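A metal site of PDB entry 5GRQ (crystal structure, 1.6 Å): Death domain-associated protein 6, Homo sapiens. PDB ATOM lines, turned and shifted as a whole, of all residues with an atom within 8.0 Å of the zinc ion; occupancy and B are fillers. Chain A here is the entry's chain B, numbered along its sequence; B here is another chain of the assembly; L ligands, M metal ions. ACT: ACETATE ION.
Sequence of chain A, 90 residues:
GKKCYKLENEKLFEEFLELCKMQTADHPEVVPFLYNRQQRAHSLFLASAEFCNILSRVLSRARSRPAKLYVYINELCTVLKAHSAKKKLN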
ATOM      1  N   PHE A  45      -5.212 -11.349  28.467  1.00  0.00           N
ATOM      2  CA  PHE A  45      -5.303 -12.781  28.752  1.00  0.00           C
ATOM      3  C   PHE A  45      -5.487 -13.039  30.246  1.00  0.00           C
ATOM      4  O   PHE A  45      -6.318 -13.850  30.648  1.00  0.00           O
ATOM      5  CB  PHE A  45      -4.048 -13.505  28.254  1.00  0.00           C
ATOM      6  CG  PHE A  45      -4.057 -14.982  28.562  1.00  0.00           C
ATOM      7  CD1 PHE A  45      -4.826 -15.840  27.803  1.00  0.00           C
ATOM      8  CD2 PHE A  45      -3.296 -15.496  29.611  1.00  0.00           C
ATOM      9  CE1 PHE A  45      -4.826 -17.207  28.074  1.00  0.00           C
ATOM     10  CE2 PHE A  45      -3.296 -16.864  29.883  1.00  0.00           C
ATOM     11  CZ  PHE A  45      -4.066 -17.722  29.114  1.00  0.00           C
ATOM     12  N   SER A  48      -9.132 -12.716  31.326  1.00  0.00           N
ATOM     13  CA  SER A  48     -10.058 -13.259  30.331  1.00  0.00           C
ATOM     14  C   SER A  48     -10.819 -14.481  30.832  1.00  0.00           C
ATOM     15  O   SER A  48     -10.364 -15.207  31.709  1.00  0.00           O
ATOM     16  CB  SER A  48      -9.303 -13.630  29.061  1.00  0.00           C
ATOM     17  OG  SER A  48      -8.441 -14.739  29.273  1.00  0.00           O
ATOM     18  N   GLU A  50     -11.164 -16.875  28.786  1.00  0.00           N
ATOM     19  CA  GLU A  50     -10.291 -17.913  28.239  1.00  0.00           C
ATOM     20  C   GLU A  50      -9.353 -18.475  29.296  1.00  0.00           C
ATOM     21  O   GLU A  50      -9.259 -19.694  29.477  1.00  0.00           O
ATOM     22  CB  GLU A  50      -9.506 -17.331  27.065  1.00  0.00           C
ATOM     23  CG  GLU A  50      -8.474 -18.299  26.479  1.00  0.00           C
ATOM     24  CD  GLU A  50      -7.511 -17.650  25.516  1.00  0.00           C
ATOM     25  OE1 GLU A  50      -7.343 -16.407  25.539  1.00  0.00           O
ATOM     26  OE2 GLU A  50      -6.883 -18.400  24.748  1.00  0.00           O
ATOM     27  N   PHE A  51      -8.669 -17.585  30.031  1.00  0.00           N
ATOM     28  CA  PHE A  51      -7.750 -18.054  31.070  1.00  0.00           C
ATOM     29  C   PHE A  51      -8.499 -18.696  32.234  1.00  0.00           C
ATOM     30  O   PHE A  51      -8.030 -19.689  32.801  1.00  0.00           O
ATOM     31  CB  PHE A  51      -6.886 -16.884  31.534  1.00  0.00           C
ATOM     32  CG  PHE A  51      -5.692 -17.283  32.378  1.00  0.00           C
ATOM     33  CD1 PHE A  51      -5.086 -18.526  32.222  1.00  0.00           C
ATOM     34  CD2 PHE A  51      -5.170 -16.397  33.306  1.00  0.00           C
ATOM     35  CE1 PHE A  51      -3.977 -18.870  32.994  1.00  0.00           C
ATOM     36  CE2 PHE A  51      -4.061 -16.742  34.088  1.00  0.00           C
ATOM     37  CZ  PHE A  51      -3.474 -17.972  33.922  1.00  0.00           C
ATOM     38  N   ILE A  54      -9.288 -22.201  31.209  1.00  0.00           N
ATOM     39  CA  ILE A  54      -8.039 -22.955  31.221  1.00  0.00           C
ATOM     40  C   ILE A  54      -7.680 -23.383  32.645  1.00  0.00           C
ATOM     41  O   ILE A  54      -7.318 -24.551  32.881  1.00  0.00           O
ATOM     42  CB  ILE A  54      -6.918 -22.136  30.563  1.00  0.00           C
ATOM     43  CG1 ILE A  54      -7.080 -22.195  29.040  1.00  0.00           C
ATOM     44  CG2 ILE A  54      -5.526 -22.625  30.982  1.00  0.00           C
ATOM     45  CD1 ILE A  54      -6.306 -21.125  28.284  1.00  0.00           C
ATOM     46  N   VAL A  79       0.904 -22.521  27.235  1.00  0.00           N
ATOM     47  CA  VAL A  79      -0.187 -21.557  27.038  1.00  0.00           C
ATOM     48  C   VAL A  79       0.236 -20.170  27.528  1.00  0.00           C
ATOM     49  O   VAL A  79       0.023 -19.165  26.843  1.00  0.00           O
ATOM     50  CB  VAL A  79      -1.457 -22.048  27.751  1.00  0.00           C
ATOM     51  CG1 VAL A  79      -2.479 -20.919  27.833  1.00  0.00           C
ATOM     52  CG2 VAL A  79      -2.023 -23.285  27.058  1.00  0.00           C
ATOM     53  N   ALA A  82       2.637 -18.579  25.155  1.00  0.00           N
ATOM     54  CA  ALA A  82       1.986 -18.150  23.918  1.00  0.00           C
ATOM     55  C   ALA A  82       1.262 -16.825  24.081  1.00  0.00           C
ATOM     56  O   ALA A  82       1.022 -16.135  23.082  1.00  0.00           O
ATOM     57  CB  ALA A  82       0.995 -19.221  23.451  1.00  0.00           C
ATOM     58  N   HIS A  83       0.873 -16.460  25.308  1.00  0.00           N
ATOM     59  CA  HIS A  83       0.202 -15.198  25.581  1.00  0.00           C
ATOM     60  C   HIS A  83       1.151 -14.200  26.254  1.00  0.00           C
ATOM     61  O   HIS A  83       0.692 -13.270  26.926  1.00  0.00           O
ATOM     62  CB  HIS A  83      -1.040 -15.454  26.425  1.00  0.00           C
ATOM     63  CG  HIS A  83      -2.089 -16.278  25.734  1.00  0.00           C
ATOM     64  ND1 HIS A  83      -2.065 -17.653  25.716  1.00  0.00           N
ATOM     65  CD2 HIS A  83      -3.181 -15.913  25.034  1.00  0.00           C
ATOM     66  CE1 HIS A  83      -3.111 -18.105  25.039  1.00  0.00           C
ATOM     67  NE2 HIS A  83      -3.815 -17.065  24.622  1.00  0.00           N
ATOM     68  N   GLY B   1      -5.790 -15.503  22.770  1.00  0.00           N
ATOM     69  CA  GLY B   1      -7.163 -15.109  22.569  1.00  0.00           C
ATOM     70  C   GLY B   1      -7.217 -13.793  21.822  1.00  0.00           C
ATOM     71  O   GLY B   1      -6.457 -13.574  20.884  1.00  0.00           O
ATOM     72  N   LYS B   2      -8.097 -12.908  22.242  1.00  0.00           N
ATOM     73  CA  LYS B   2      -8.197 -11.619  21.573  1.00  0.00           C
ATOM     74  C   LYS B   2      -6.932 -10.791  21.783  1.00  0.00           C
ATOM     75  O   LYS B   2      -6.142 -11.022  22.704  1.00  0.00           O
ATOM     76  CB  LYS B   2      -9.442 -10.889  22.040  1.00  0.00           C
ATOM     77  CG  LYS B   2     -10.699 -11.546  21.436  1.00  0.00           C
ATOM     78  CD  LYS B   2     -12.013 -11.019  21.953  1.00  0.00           C
ATOM     79  CE  LYS B   2     -13.154 -11.747  21.261  1.00  0.00           C
ATOM     80  NZ  LYS B   2     -14.471 -11.512  21.928  1.00  0.00           N
HETATM   81  C   ACT L   1      -6.018 -18.842  21.457  1.00  0.00           C
HETATM   82  O   ACT L   1      -7.154 -18.312  21.522  1.00  0.00           O
HETATM   83  OXT ACT L   1      -5.038 -18.683  22.201  1.00  0.00           O
HETATM   84  CH3 ACT L   1      -5.816 -19.849  20.279  1.00  0.00           C
HETATM   85 ZN    ZN M   1      -5.567 -17.301  23.618  1.00  0.00          ZN
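Of the 10 residues printed, 3 come within 4 Å of the zinc ion. The nearest printed residue that does not touch the zinc ion is Phe 45 (4.5 Å).
A ring nitrogen (ND1) of His 83 lies within hydrogen-bond range of the backbone carbonyl oxygen (O) of Val 79 (2.8 Å). N of Glu 50 sits close to OG of Ser 48, at 3.5 Å.
The zinc ion is bound by N of Gly 1 of chain B, NE2 of His 83, OXT of the ligand and OE2 of Glu 50. Slightly farther from the zinc ion lies OE1 of Glu 50 (2.8 Å). Slightly farther from the zinc ion lies O of the ligand (2.8 Å).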
